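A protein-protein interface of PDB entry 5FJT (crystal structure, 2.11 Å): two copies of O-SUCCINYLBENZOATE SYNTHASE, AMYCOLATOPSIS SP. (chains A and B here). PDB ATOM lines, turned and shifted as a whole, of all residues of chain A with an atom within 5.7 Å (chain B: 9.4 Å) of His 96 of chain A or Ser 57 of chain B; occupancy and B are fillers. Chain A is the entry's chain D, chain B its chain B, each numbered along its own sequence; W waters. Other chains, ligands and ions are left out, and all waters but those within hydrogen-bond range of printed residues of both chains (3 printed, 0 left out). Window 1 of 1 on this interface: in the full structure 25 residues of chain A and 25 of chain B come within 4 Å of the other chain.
The side-chain carboxylate of Glu 220 of chain B is in salt-bridge range of the guanidinium group of Arg 97 of chain A, 2.7 Å away.
N of Lys 94 of chain A lies within hydrogen-bond range of O of Pro 53 of chain B (2.9 Å).
NE2 of His 96 of chain B lies within hydrogen-bond range of O of Ser 57 of chain A (2.9 Å).
O of Ser 57 of chain B is in hydrogen-bond range of NE2 of His 96 of chain A, at 2.9 Å.
The backbone NH (N) of Arg 97 of chain A is in hydrogen-bond range of the side-chain carboxylate (OE2) of Glu 58 of chain A, at 3.3 Å.
The side-chain hydroxyl (OG) of Ser 56 of chain B lies close to the backbone NH (N) of Glu 58 of chain B, at 3.4 Å.
The backbone NH of Leu 71 of chain A is in hydrogen-bond range of the backbone carbonyl oxygen of Val 66 of chain A, at 3.0 Å.
CA of Ser 57 of chain A touches O of Lys 94 of chain B (3.4 Å).
Val 66 of chain A touches Tyr 59 of chain B.
Lys 94 of chain A touches Leu 54 of chain B (CE to O, 3.5 Å).
Tyr 55 of chain B touches Lys 94 of chain A.
Ser 56 of chain B touches Lys 94 of chain A.
Ser 57 of chain B touches Lys 94 of chain A (CA to O, 3.4 Å).
NE2 of His 96 of chain A touches CE1 of Tyr 59 of chain B, at 3.95 Å.
Of the printed residues of chain B, Ser 57 of chain A touches Lys 94 (3.4 Å) and His 96 (2.9 Å).
Printed residues of chain B within 4 Å of Lys 94 of chain A: Pro 53, Leu 54, Tyr 55, Ser 56 and Ser 57.
No residue of chain B comes within 4 Å of Gly 95 of chain A.
Printed residues of chain B within 4 Å of His 96 of chain A: Ser 57 and Tyr 59.
No residue of chain B comes within 4 Å of Ala 99 of chain A.
Printed residues of chain A within 4 Å of Leu 54 of chain B: Lys 94 (3.5 Å).
Ser 57 of chain B touches two residues of chain A.
Printed residues of chain A within 4 Å of Glu 220 of chain B: Arg 97.
The nearest printed residue of chain A that does not touch Pro 53 of chain B is His 96 of chain A (4.4 Å).
Of the 14 printed residues of chain A, 5 touch a printed residue of chain B.
Hydrophobic or aromatic side chains of chain A within 4 Å of the printed part of chain B: Val 66 and His 96.
Hydrophobic or aromatic side chains of chain B within 4 Å of the printed part of chain A: Tyr 59 and His 96.
Among the printed residues, 11 pairs touch across the chains.
Among the printed residues, Asp or Glu carboxylates within 4 Å of a Lys or Arg side-chain nitrogen of the other chain: Arg 97 of chain A with Glu 220 of chain B.
Ser 57 of chain A touches Lys 94 of chain B, and with the chains exchanged Lys 94 of chain A touches Ser 57 of chain B.
Ser 57 of chain A touches His 96 of chain B, and with the chains exchanged His 96 of chain A touches Ser 57 of chain B.
Positions printed for both chains: 57, 58, 62, 63, 94, 95, 96, 97 and 98.
Of the 11 pairs that touch across the chains among the printed residues, 4 have their exchanged pair printed and touching as well.
Water W1 bridges OH of Tyr 59 of chain B and O of Gly 62 of chain A.
Water W2 bridges N of Glu 219 of chain B (2.9 Å) and NZ of Lys 94 of chain A (3.1 Å).
Water W3 bridges O of Leu 54 of chain B (3.0 Å) and NZ of Lys 94 of chain A (3.4 Å).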
ATOM      1  N   SER A  57      21.473 -15.710  34.864  1.00  0.00           N
ATOM      2  CA  SER A  57      20.932 -16.136  33.581  1.00  0.00           C
ATOM      3  C   SER A  57      22.020 -16.463  32.524  1.00  0.00           C
ATOM      4  O   SER A  57      21.713 -17.100  31.505  1.00  0.00           O
ATOM      5  CB  SER A  57      19.950 -15.075  33.091  1.00  0.00           C
ATOM      6  OG  SER A  57      20.639 -13.902  32.726  1.00  0.00           O
ATOM      7  N   GLU A  58      23.221 -15.936  32.725  1.00  0.00           N
ATOM      8  CA  GLU A  58      24.285 -16.084  31.766  1.00  0.00           C
ATOM      9  C   GLU A  58      24.984 -17.442  31.981  1.00  0.00           C
ATOM     10  O   GLU A  58      25.036 -17.953  33.078  1.00  0.00           O
ATOM     11  CB  GLU A  58      25.315 -15.002  31.898  1.00  0.00           C
ATOM     12  CG  GLU A  58      24.793 -13.660  31.464  1.00  0.00           C
ATOM     13  CD  GLU A  58      25.904 -12.610  31.519  1.00  0.00           C
ATOM     14  OE1 GLU A  58      26.698 -12.543  30.516  1.00  0.00           O
ATOM     15  OE2 GLU A  58      25.990 -11.886  32.587  1.00  0.00           O
ATOM     16  N   GLY A  62      25.940 -19.461  26.129  1.00  0.00           N
ATOM     17  CA  GLY A  62      25.257 -18.184  25.871  1.00  0.00           C
ATOM     18  C   GLY A  62      26.230 -17.038  25.726  1.00  0.00           C
ATOM     19  O   GLY A  62      26.094 -16.170  24.841  1.00  0.00           O
ATOM     20  N   ALA A  63      27.196 -16.982  26.624  1.00  0.00           N
ATOM     21  CA  ALA A  63      28.207 -15.903  26.568  1.00  0.00           C
ATOM     22  C   ALA A  63      29.049 -16.007  25.272  1.00  0.00           C
ATOM     23  O   ALA A  63      29.340 -15.005  24.554  1.00  0.00           O
ATOM     24  CB  ALA A  63      29.106 -15.993  27.768  1.00  0.00           C
ATOM     25  N   VAL A  66      26.874 -14.715  22.337  1.00  0.00           N
ATOM     26  CA  VAL A  66      26.663 -13.249  22.247  1.00  0.00           C
ATOM     27  C   VAL A  66      28.000 -12.560  21.922  1.00  0.00           C
ATOM     28  O   VAL A  66      28.001 -11.582  21.231  1.00  0.00           O
ATOM     29  CB  VAL A  66      25.953 -12.672  23.526  1.00  0.00           C
ATOM     30  CG1 VAL A  66      26.899 -12.548  24.683  1.00  0.00           C
ATOM     31  CG2 VAL A  66      25.330 -11.338  23.275  1.00  0.00           C
ATOM     32  N   LEU A  71      28.882  -8.883  20.380  1.00  0.00           N
ATOM     33  CA  LEU A  71      29.812  -7.985  21.097  1.00  0.00           C
ATOM     34  C   LEU A  71      31.175  -7.808  20.401  1.00  0.00           C
ATOM     35  O   LEU A  71      31.667  -6.685  20.257  1.00  0.00           O
ATOM     36  CB  LEU A  71      30.041  -8.465  22.522  1.00  0.00           C
ATOM     37  CG  LEU A  71      28.764  -8.786  23.353  1.00  0.00           C
ATOM     38  CD1 LEU A  71      29.227  -9.118  24.771  1.00  0.00           C
ATOM     39  CD2 LEU A  71      27.828  -7.626  23.328  1.00  0.00           C
ATOM     40  N   LYS A  94      21.420  -5.332  25.528  1.00  0.00           N
ATOM     41  CA  LYS A  94      20.923  -5.384  26.892  1.00  0.00           C
ATOM     42  C   LYS A  94      21.509  -6.515  27.645  1.00  0.00           C
ATOM     43  O   LYS A  94      21.577  -7.646  27.128  1.00  0.00           O
ATOM     44  CB  LYS A  94      19.435  -5.603  26.907  1.00  0.00           C
ATOM     45  CG  LYS A  94      18.642  -4.465  26.268  1.00  0.00           C
ATOM     46  CD  LYS A  94      18.715  -3.135  27.037  1.00  0.00           C
ATOM     47  CE  LYS A  94      17.581  -2.197  26.536  1.00  0.00           C
ATOM     48  NZ  LYS A  94      17.711  -0.830  27.077  1.00  0.00           N
ATOM     49  N   GLY A  95      21.904  -6.272  28.880  1.00  0.00           N
ATOM     50  CA  GLY A  95      22.385  -7.349  29.746  1.00  0.00           C
ATOM     51  C   GLY A  95      23.725  -7.940  29.284  1.00  0.00           C
ATOM     52  O   GLY A  95      24.627  -7.199  28.861  1.00  0.00           O
ATOM     53  N   HIS A  96      23.880  -9.269  29.447  1.00  0.00           N
ATOM     54  CA  HIS A  96      25.128  -9.950  29.118  1.00  0.00           C
ATOM     55  C   HIS A  96      26.383  -9.355  29.751  1.00  0.00           C
ATOM     56  O   HIS A  96      27.454  -9.245  29.111  1.00  0.00           O
ATOM     57  CB  HIS A  96      25.275 -10.048  27.583  1.00  0.00           C
ATOM     58  CG  HIS A  96      24.166 -10.824  26.972  1.00  0.00           C
ATOM     59  ND1 HIS A  96      24.141 -12.192  27.008  1.00  0.00           N
ATOM     60  CD2 HIS A  96      22.976 -10.433  26.457  1.00  0.00           C
ATOM     61  CE1 HIS A  96      22.998 -12.623  26.498  1.00  0.00           C
ATOM     62  NE2 HIS A  96      22.253 -11.569  26.204  1.00  0.00           N
ATOM     63  N   ARG A  97      26.245  -9.015  31.041  1.00  0.00           N
ATOM     64  CA  ARG A  97      27.271  -8.329  31.745  1.00  0.00           C
ATOM     65  C   ARG A  97      28.538  -9.130  31.871  1.00  0.00           C
ATOM     66  O   ARG A  97      29.631  -8.583  31.786  1.00  0.00           O
ATOM     67  CB  ARG A  97      26.792  -7.920  33.150  1.00  0.00           C
ATOM     68  CG  ARG A  97      25.818  -6.762  33.082  1.00  0.00           C
ATOM     69  CD  ARG A  97      25.483  -6.292  34.488  1.00  0.00           C
ATOM     70  NE  ARG A  97      24.734  -5.030  34.428  1.00  0.00           N
ATOM     71  CZ  ARG A  97      23.421  -4.901  34.441  1.00  0.00           C
ATOM     72  NH1 ARG A  97      22.616  -5.925  34.584  1.00  0.00           N
ATOM     73  NH2 ARG A  97      22.929  -3.670  34.422  1.00  0.00           N
ATOM     74  N   MET A  98      28.412 -10.408  32.193  1.00  0.00           N
ATOM     75  CA  MET A  98      29.622 -11.208  32.371  1.00  0.00           C
ATOM     76  C   MET A  98      30.426 -11.331  31.045  1.00  0.00           C
ATOM     77  O   MET A  98      31.630 -11.287  31.059  1.00  0.00           O
ATOM     78  CB  MET A  98      29.272 -12.613  32.881  1.00  0.00           C
ATOM     79  CG  MET A  98      28.737 -12.613  34.284  1.00  0.00           C
ATOM     80  SD  MET A  98      28.135 -14.217  34.824  1.00  0.00           S
ATOM     81  CE  MET A  98      27.770 -13.851  36.568  1.00  0.00           C
ATOM     82  N   ALA A  99      29.694 -11.523  29.941  1.00  0.00           N
ATOM     83  CA  ALA A  99      30.318 -11.551  28.615  1.00  0.00           C
ATOM     84  C   ALA A  99      30.995 -10.229  28.291  1.00  0.00           C
ATOM     85  O   ALA A  99      32.158 -10.192  27.839  1.00  0.00           O
ATOM     86  CB  ALA A  99      29.301 -11.907  27.557  1.00  0.00           C
ATOM     87  N   LYS A 100      30.282  -9.123  28.491  1.00  0.00           N
ATOM     88  CA  LYS A 100      30.884  -7.799  28.277  1.00  0.00           C
ATOM     89  C   LYS A 100      32.100  -7.547  29.139  1.00  0.00           C
ATOM     90  O   LYS A 100      33.108  -6.969  28.686  1.00  0.00           O
ATOM     91  CB  LYS A 100      29.875  -6.650  28.555  1.00  0.00           C
ATOM     92  CG  LYS A 100      28.724  -6.575  27.540  1.00  0.00           C
ATOM     93  CD  LYS A 100      27.817  -5.408  27.905  1.00  0.00           C
ATOM     94  CE  LYS A 100      26.642  -5.326  26.995  1.00  0.00           C
ATOM     95  NZ  LYS A 100      25.832  -4.114  27.277  1.00  0.00           N
ATOM     96  N   GLY A 101      31.998  -7.948  30.401  1.00  0.00           N
ATOM     97  CA  GLY A 101      33.111  -7.792  31.354  1.00  0.00           C
ATOM     98  C   GLY A 101      34.407  -8.513  30.899  1.00  0.00           C
ATOM     99  O   GLY A 101      35.512  -8.021  31.110  1.00  0.00           O
ATOM    100  N   THR B  49      10.805 -13.149  21.780  1.00  0.00           N
ATOM    101  CA  THR B  49      12.138 -12.630  21.448  1.00  0.00           C
ATOM    102  C   THR B  49      12.212 -12.100  20.030  1.00  0.00           C
ATOM    103  O   THR B  49      11.413 -12.461  19.153  1.00  0.00           O
ATOM    104  CB  THR B  49      13.238 -13.687  21.609  1.00  0.00           C
ATOM    105  OG1 THR B  49      12.792 -14.952  21.117  1.00  0.00           O
ATOM    106  CG2 THR B  49      13.530 -13.875  23.092  1.00  0.00           C
ATOM    107  N   MET B  50      13.198 -11.248  19.828  1.00  0.00           N
ATOM    108  CA  MET B  50      13.612 -10.763  18.512  1.00  0.00           C
ATOM    109  C   MET B  50      14.955 -11.360  18.177  1.00  0.00           C
ATOM    110  O   MET B  50      15.524 -12.083  18.964  1.00  0.00           O
ATOM    111  CB  MET B  50      13.714  -9.238  18.547  1.00  0.00           C
ATOM    112  CG  MET B  50      12.382  -8.536  18.617  1.00  0.00           C
ATOM    113  SD  MET B  50      12.703  -6.801  19.113  1.00  0.00           S
ATOM    114  CE  MET B  50      14.419  -6.426  18.748  1.00  0.00           C
ATOM    115  N   ALA B  51      15.510 -10.996  17.021  1.00  0.00           N
ATOM    116  CA  ALA B  51      16.741 -11.594  16.565  1.00  0.00           C
ATOM    117  C   ALA B  51      17.932 -11.257  17.447  1.00  0.00           C
ATOM    118  O   ALA B  51      18.798 -12.110  17.679  1.00  0.00           O
ATOM    119  CB  ALA B  51      17.044 -11.139  15.088  1.00  0.00           C
ATOM    120  N   GLY B  52      18.019 -10.007  17.932  1.00  0.00           N
ATOM    121  CA  GLY B  52      19.124  -9.597  18.795  1.00  0.00           C
ATOM    122  C   GLY B  52      18.647  -8.979  20.109  1.00  0.00           C
ATOM    123  O   GLY B  52      17.443  -8.626  20.233  1.00  0.00           O
ATOM    124  N   PRO B  53      19.550  -8.839  21.079  1.00  0.00           N
ATOM    125  CA  PRO B  53      19.135  -8.403  22.432  1.00  0.00           C
ATOM    126  C   PRO B  53      19.042  -6.883  22.561  1.00  0.00           C
ATOM    127  O   PRO B  53      19.805  -6.250  23.301  1.00  0.00           O
ATOM    128  CB  PRO B  53      20.223  -8.981  23.313  1.00  0.00           C
ATOM    129  CG  PRO B  53      21.462  -8.968  22.443  1.00  0.00           C
ATOM    130  CD  PRO B  53      20.952  -9.319  21.073  1.00  0.00           C
ATOM    131  N   LEU B  54      18.074  -6.307  21.868  1.00  0.00           N
ATOM    132  CA  LEU B  54      17.930  -4.858  21.823  1.00  0.00           C
ATOM    133  C   LEU B  54      16.820  -4.335  22.755  1.00  0.00           C
ATOM    134  O   LEU B  54      16.895  -3.196  23.209  1.00  0.00           O
ATOM    135  CB  LEU B  54      17.672  -4.390  20.378  1.00  0.00           C
ATOM    136  CG  LEU B  54      18.765  -4.775  19.339  1.00  0.00           C
ATOM    137  CD1 LEU B  54      18.391  -4.207  17.956  1.00  0.00           C
ATOM    138  CD2 LEU B  54      20.152  -4.301  19.739  1.00  0.00           C
ATOM    139  N   TYR B  55      15.776  -5.119  22.969  1.00  0.00           N
ATOM    140  CA  TYR B  55      14.666  -4.769  23.836  1.00  0.00           C
ATOM    141  C   TYR B  55      14.933  -5.323  25.237  1.00  0.00           C
ATOM    142  O   TYR B  55      14.676  -4.666  26.224  1.00  0.00           O
ATOM    143  CB  TYR B  55      13.298  -5.227  23.274  1.00  0.00           C
ATOM    144  CG  TYR B  55      12.144  -5.289  24.282  1.00  0.00           C
ATOM    145  CD1 TYR B  55      11.936  -6.435  25.055  1.00  0.00           C
ATOM    146  CD2 TYR B  55      11.274  -4.204  24.480  1.00  0.00           C
ATOM    147  CE1 TYR B  55      10.906  -6.503  25.982  1.00  0.00           C
ATOM    148  CE2 TYR B  55      10.243  -4.262  25.407  1.00  0.00           C
ATOM    149  CZ  TYR B  55      10.064  -5.435  26.155  1.00  0.00           C
ATOM    150  OH  TYR B  55       9.053  -5.581  27.112  1.00  0.00           O
ATOM    151  N   SER B  56      15.413  -6.532  25.306  1.00  0.00           N
ATOM    152  CA  SER B  56      15.846  -7.137  26.541  1.00  0.00           C
ATOM    153  C   SER B  56      17.039  -8.042  26.246  1.00  0.00           C
ATOM    154  O   SER B  56      17.465  -8.135  25.118  1.00  0.00           O
ATOM    155  CB  SER B  56      14.691  -7.933  27.160  1.00  0.00           C
ATOM    156  OG  SER B  56      14.522  -9.243  26.625  1.00  0.00           O
ATOM    157  N   SER B  57      17.565  -8.708  27.264  1.00  0.00           N
ATOM    158  CA  SER B  57      18.737  -9.520  27.101  1.00  0.00           C
ATOM    159  C   SER B  57      18.485 -10.853  26.298  1.00  0.00           C
ATOM    160  O   SER B  57      19.407 -11.462  25.786  1.00  0.00           O
ATOM    161  CB  SER B  57      19.321  -9.836  28.464  1.00  0.00           C
ATOM    162  OG  SER B  57      18.487 -10.741  29.161  1.00  0.00           O
ATOM    163  N   GLU B  58      17.228 -11.244  26.207  1.00  0.00           N
ATOM    164  CA  GLU B  58      16.852 -12.466  25.522  1.00  0.00           C
ATOM    165  C   GLU B  58      16.739 -12.208  24.002  1.00  0.00           C
ATOM    166  O   GLU B  58      16.362 -11.142  23.576  1.00  0.00           O
ATOM    167  CB  GLU B  58      15.561 -13.038  26.053  1.00  0.00           C
ATOM    168  CG  GLU B  58      15.652 -13.526  27.467  1.00  0.00           C
ATOM    169  CD  GLU B  58      14.338 -14.189  27.888  1.00  0.00           C
ATOM    170  OE1 GLU B  58      14.117 -15.398  27.492  1.00  0.00           O
ATOM    171  OE2 GLU B  58      13.490 -13.459  28.516  1.00  0.00           O
ATOM    172  N   TYR B  59      17.119 -13.200  23.222  1.00  0.00           N
ATOM    173  CA  TYR B  59      16.969 -13.098  21.784  1.00  0.00           C
ATOM    174  C   TYR B  59      16.765 -14.530  21.181  1.00  0.00           C
ATOM    175  O   TYR B  59      16.949 -15.507  21.864  1.00  0.00           O
ATOM    176  CB  TYR B  59      18.139 -12.350  21.169  1.00  0.00           C
ATOM    177  CG  TYR B  59      19.478 -12.965  21.384  1.00  0.00           C
ATOM    178  CD1 TYR B  59      20.160 -12.838  22.589  1.00  0.00           C
ATOM    179  CD2 TYR B  59      20.132 -13.689  20.338  1.00  0.00           C
ATOM    180  CE1 TYR B  59      21.438 -13.392  22.795  1.00  0.00           C
ATOM    181  CE2 TYR B  59      21.390 -14.250  20.524  1.00  0.00           C
ATOM    182  CZ  TYR B  59      22.082 -14.075  21.703  1.00  0.00           C
ATOM    183  OH  TYR B  59      23.314 -14.634  21.897  1.00  0.00           O
ATOM    184  N   ASN B  60      16.392 -14.597  19.911  1.00  0.00           N
ATOM    185  CA  ASN B  60      15.916 -15.879  19.326  1.00  0.00           C
ATOM    186  C   ASN B  60      16.873 -17.036  19.469  1.00  0.00           C
ATOM    187  O   ASN B  60      16.483 -18.062  19.963  1.00  0.00           O
ATOM    188  CB  ASN B  60      15.509 -15.673  17.850  1.00  0.00           C
ATOM    189  CG  ASN B  60      14.275 -14.847  17.694  1.00  0.00           C
ATOM    190  OD1 ASN B  60      13.373 -14.846  18.540  1.00  0.00           O
ATOM    191  ND2 ASN B  60      14.142 -14.226  16.535  1.00  0.00           N
ATOM    192  N   ASP B  61      18.145 -16.871  19.105  1.00  0.00           N
ATOM    193  CA  ASP B  61      19.066 -17.976  19.187  1.00  0.00           C
ATOM    194  C   ASP B  61      19.329 -18.341  20.619  1.00  0.00           C
ATOM    195  O   ASP B  61      19.516 -19.519  20.936  1.00  0.00           O
ATOM    196  CB  ASP B  61      20.428 -17.690  18.543  1.00  0.00           C
ATOM    197  CG  ASP B  61      20.399 -17.661  16.978  1.00  0.00           C
ATOM    198  OD1 ASP B  61      19.397 -18.034  16.363  1.00  0.00           O
ATOM    199  OD2 ASP B  61      21.362 -17.175  16.389  1.00  0.00           O
ATOM    200  N   GLY B  62      19.356 -17.344  21.515  1.00  0.00           N
ATOM    201  CA  GLY B  62      19.541 -17.663  22.946  1.00  0.00           C
ATOM    202  C   GLY B  62      18.353 -18.425  23.529  1.00  0.00           C
ATOM    203  O   GLY B  62      18.534 -19.368  24.266  1.00  0.00           O
ATOM    204  N   ALA B  63      17.150 -18.031  23.151  1.00  0.00           N
ATOM    205  CA  ALA B  63      15.936 -18.699  23.633  1.00  0.00           C
ATOM    206  C   ALA B  63      15.868 -20.126  23.105  1.00  0.00           C
ATOM    207  O   ALA B  63      15.588 -21.129  23.823  1.00  0.00           O
ATOM    208  CB  ALA B  63      14.729 -17.943  23.196  1.00  0.00           C
ATOM    209  N   LYS B  94      17.850 -19.612  36.104  1.00  0.00           N
ATOM    210  CA  LYS B  94      17.654 -18.156  36.336  1.00  0.00           C
ATOM    211  C   LYS B  94      17.305 -17.442  35.067  1.00  0.00           C
ATOM    212  O   LYS B  94      17.924 -17.645  34.035  1.00  0.00           O
ATOM    213  CB  LYS B  94      18.917 -17.517  36.858  1.00  0.00           C
ATOM    214  CG  LYS B  94      19.424 -18.059  38.171  1.00  0.00           C
ATOM    215  CD  LYS B  94      18.517 -17.727  39.356  1.00  0.00           C
ATOM    216  CE  LYS B  94      19.330 -17.974  40.642  1.00  0.00           C
ATOM    217  NZ  LYS B  94      18.508 -17.853  41.874  1.00  0.00           N
ATOM    218  N   GLY B  95      16.318 -16.580  35.144  1.00  0.00           N
ATOM    219  CA  GLY B  95      15.941 -15.732  34.035  1.00  0.00           C
ATOM    220  C   GLY B  95      15.283 -16.491  32.867  1.00  0.00           C
ATOM    221  O   GLY B  95      14.504 -17.389  33.113  1.00  0.00           O
ATOM    222  N   HIS B  96      15.598 -16.068  31.631  1.00  0.00           N
ATOM    223  CA  HIS B  96      15.018 -16.661  30.450  1.00  0.00           C
ATOM    224  C   HIS B  96      13.535 -16.743  30.497  1.00  0.00           C
ATOM    225  O   HIS B  96      12.896 -17.746  30.035  1.00  0.00           O
ATOM    226  CB  HIS B  96      15.633 -18.066  30.208  1.00  0.00           C
ATOM    227  CG  HIS B  96      17.092 -17.999  29.980  1.00  0.00           C
ATOM    228  ND1 HIS B  96      17.623 -17.646  28.758  1.00  0.00           N
ATOM    229  CD2 HIS B  96      18.128 -18.075  30.840  1.00  0.00           C
ATOM    230  CE1 HIS B  96      18.933 -17.566  28.865  1.00  0.00           C
ATOM    231  NE2 HIS B  96      19.269 -17.854  30.112  1.00  0.00           N
ATOM    232  N   ARG B  97      12.953 -15.629  30.892  1.00  0.00           N
ATOM    233  CA  ARG B  97      11.519 -15.554  31.047  1.00  0.00           C
ATOM    234  C   ARG B  97      10.746 -15.732  29.764  1.00  0.00           C
ATOM    235  O   ARG B  97       9.671 -16.353  29.780  1.00  0.00           O
ATOM    236  CB  ARG B  97      11.115 -14.216  31.699  1.00  0.00           C
ATOM    237  CG  ARG B  97      11.511 -14.187  33.192  1.00  0.00           C
ATOM    238  CD  ARG B  97      10.967 -12.926  33.843  1.00  0.00           C
ATOM    239  NE  ARG B  97      11.086 -13.019  35.298  1.00  0.00           N
ATOM    240  CZ  ARG B  97      12.065 -12.475  36.029  1.00  0.00           C
ATOM    241  NH1 ARG B  97      13.046 -11.808  35.491  1.00  0.00           N
ATOM    242  NH2 ARG B  97      12.010 -12.613  37.344  1.00  0.00           N
ATOM    243  N   MET B  98      11.169 -15.072  28.693  1.00  0.00           N
ATOM    244  CA  MET B  98      10.409 -15.176  27.449  1.00  0.00           C
ATOM    245  C   MET B  98      10.396 -16.637  26.946  1.00  0.00           C
ATOM    246  O   MET B  98       9.378 -17.093  26.429  1.00  0.00           O
ATOM    247  CB  MET B  98      10.998 -14.272  26.388  1.00  0.00           C
ATOM    248  CG  MET B  98      10.812 -12.803  26.706  1.00  0.00           C
ATOM    249  SD  MET B  98      11.648 -11.703  25.574  1.00  0.00           S
ATOM    250  CE  MET B  98      11.051 -10.089  26.156  1.00  0.00           C
ATOM    251  N   GLU B 219      15.395  -0.268  32.260  1.00  0.00           N
ATOM    252  CA  GLU B 219      14.672  -1.403  32.863  1.00  0.00           C
ATOM    253  C   GLU B 219      14.909  -1.536  34.364  1.00  0.00           C
ATOM    254  O   GLU B 219      13.985  -1.751  35.160  1.00  0.00           O
ATOM    255  CB  GLU B 219      15.131  -2.777  32.136  1.00  0.00           C
ATOM    256  CG  GLU B 219      14.604  -4.038  32.815  1.00  0.00           C
ATOM    257  CD  GLU B 219      15.046  -5.413  32.193  1.00  0.00           C
ATOM    258  OE1 GLU B 219      15.137  -5.518  30.961  1.00  0.00           O
ATOM    259  OE2 GLU B 219      15.259  -6.396  32.958  1.00  0.00           O
ATOM    260  N   GLU B 220      16.152  -1.472  34.749  1.00  0.00           N
ATOM    261  CA  GLU B 220      16.510  -1.665  36.142  1.00  0.00           C
ATOM    262  C   GLU B 220      16.341  -0.401  37.030  1.00  0.00           C
ATOM    263  O   GLU B 220      16.526  -0.475  38.252  1.00  0.00           O
ATOM    264  CB  GLU B 220      17.973  -2.141  36.237  1.00  0.00           C
ATOM    265  CG  GLU B 220      18.133  -3.578  35.727  1.00  0.00           C
ATOM    266  CD  GLU B 220      19.591  -3.930  35.364  1.00  0.00           C
ATOM    267  OE1 GLU B 220      20.348  -3.021  35.032  1.00  0.00           O
ATOM    268  OE2 GLU B 220      19.946  -5.127  35.345  1.00  0.00           O
ATOM    269  N   GLU B 240       9.246  -2.689  30.314  1.00  0.00           N
ATOM    270  CA  GLU B 240      10.462  -3.475  30.489  1.00  0.00           C
ATOM    271  C   GLU B 240      10.770  -3.804  31.970  1.00  0.00           C
ATOM    272  O   GLU B 240      11.255  -4.904  32.276  1.00  0.00           O
ATOM    273  CB  GLU B 240      11.703  -2.782  29.872  1.00  0.00           C
ATOM    274  CG  GLU B 240      11.841  -2.834  28.357  1.00  0.00           C
ATOM    275  CD  GLU B 240      11.098  -1.706  27.622  1.00  0.00           C
ATOM    276  OE1 GLU B 240      10.020  -1.293  28.100  1.00  0.00           O
ATOM    277  OE2 GLU B 240      11.588  -1.251  26.555  1.00  0.00           O
ATOM    278  N   VAL B 243       8.945  -7.386  35.291  1.00  0.00           N
ATOM    279  CA  VAL B 243       9.356  -8.738  34.902  1.00  0.00           C
ATOM    280  C   VAL B 243       8.660  -9.824  35.655  1.00  0.00           C
ATOM    281  O   VAL B 243       8.824 -10.978  35.323  1.00  0.00           O
ATOM    282  CB  VAL B 243      10.871  -8.941  35.073  1.00  0.00           C
ATOM    283  CG1 VAL B 243      11.622  -8.021  34.116  1.00  0.00           C
ATOM    284  CG2 VAL B 243      11.336  -8.709  36.527  1.00  0.00           C
ATOM    285  N   ARG B 266       7.226 -11.381  28.491  1.00  0.00           N
ATOM    286  CA  ARG B 266       8.174 -10.631  29.302  1.00  0.00           C
ATOM    287  C   ARG B 266       8.177 -11.093  30.780  1.00  0.00           C
ATOM    288  O   ARG B 266       9.206 -10.998  31.461  1.00  0.00           O
ATOM    289  CB  ARG B 266       7.851  -9.142  29.192  1.00  0.00           C
ATOM    290  CG  ARG B 266       8.829  -8.175  29.848  1.00  0.00           C
ATOM    291  CD  ARG B 266       8.183  -6.784  29.957  1.00  0.00           C
ATOM    292  NE  ARG B 266       7.093  -6.838  30.927  1.00  0.00           N
ATOM    293  CZ  ARG B 266       5.927  -6.246  30.835  1.00  0.00           C
ATOM    294  NH1 ARG B 266       5.617  -5.459  29.825  1.00  0.00           N
ATOM    295  NH2 ARG B 266       5.056  -6.415  31.810  1.00  0.00           N
HETATM  296  O   HOH W   1      23.455 -15.783  24.134  1.00  0.00           O
HETATM  297  O   HOH W   2      16.692  -1.344  29.907  1.00  0.00           O
HETATM  298  O   HOH W   3      15.749  -0.626  24.251  1.00  0.00           O
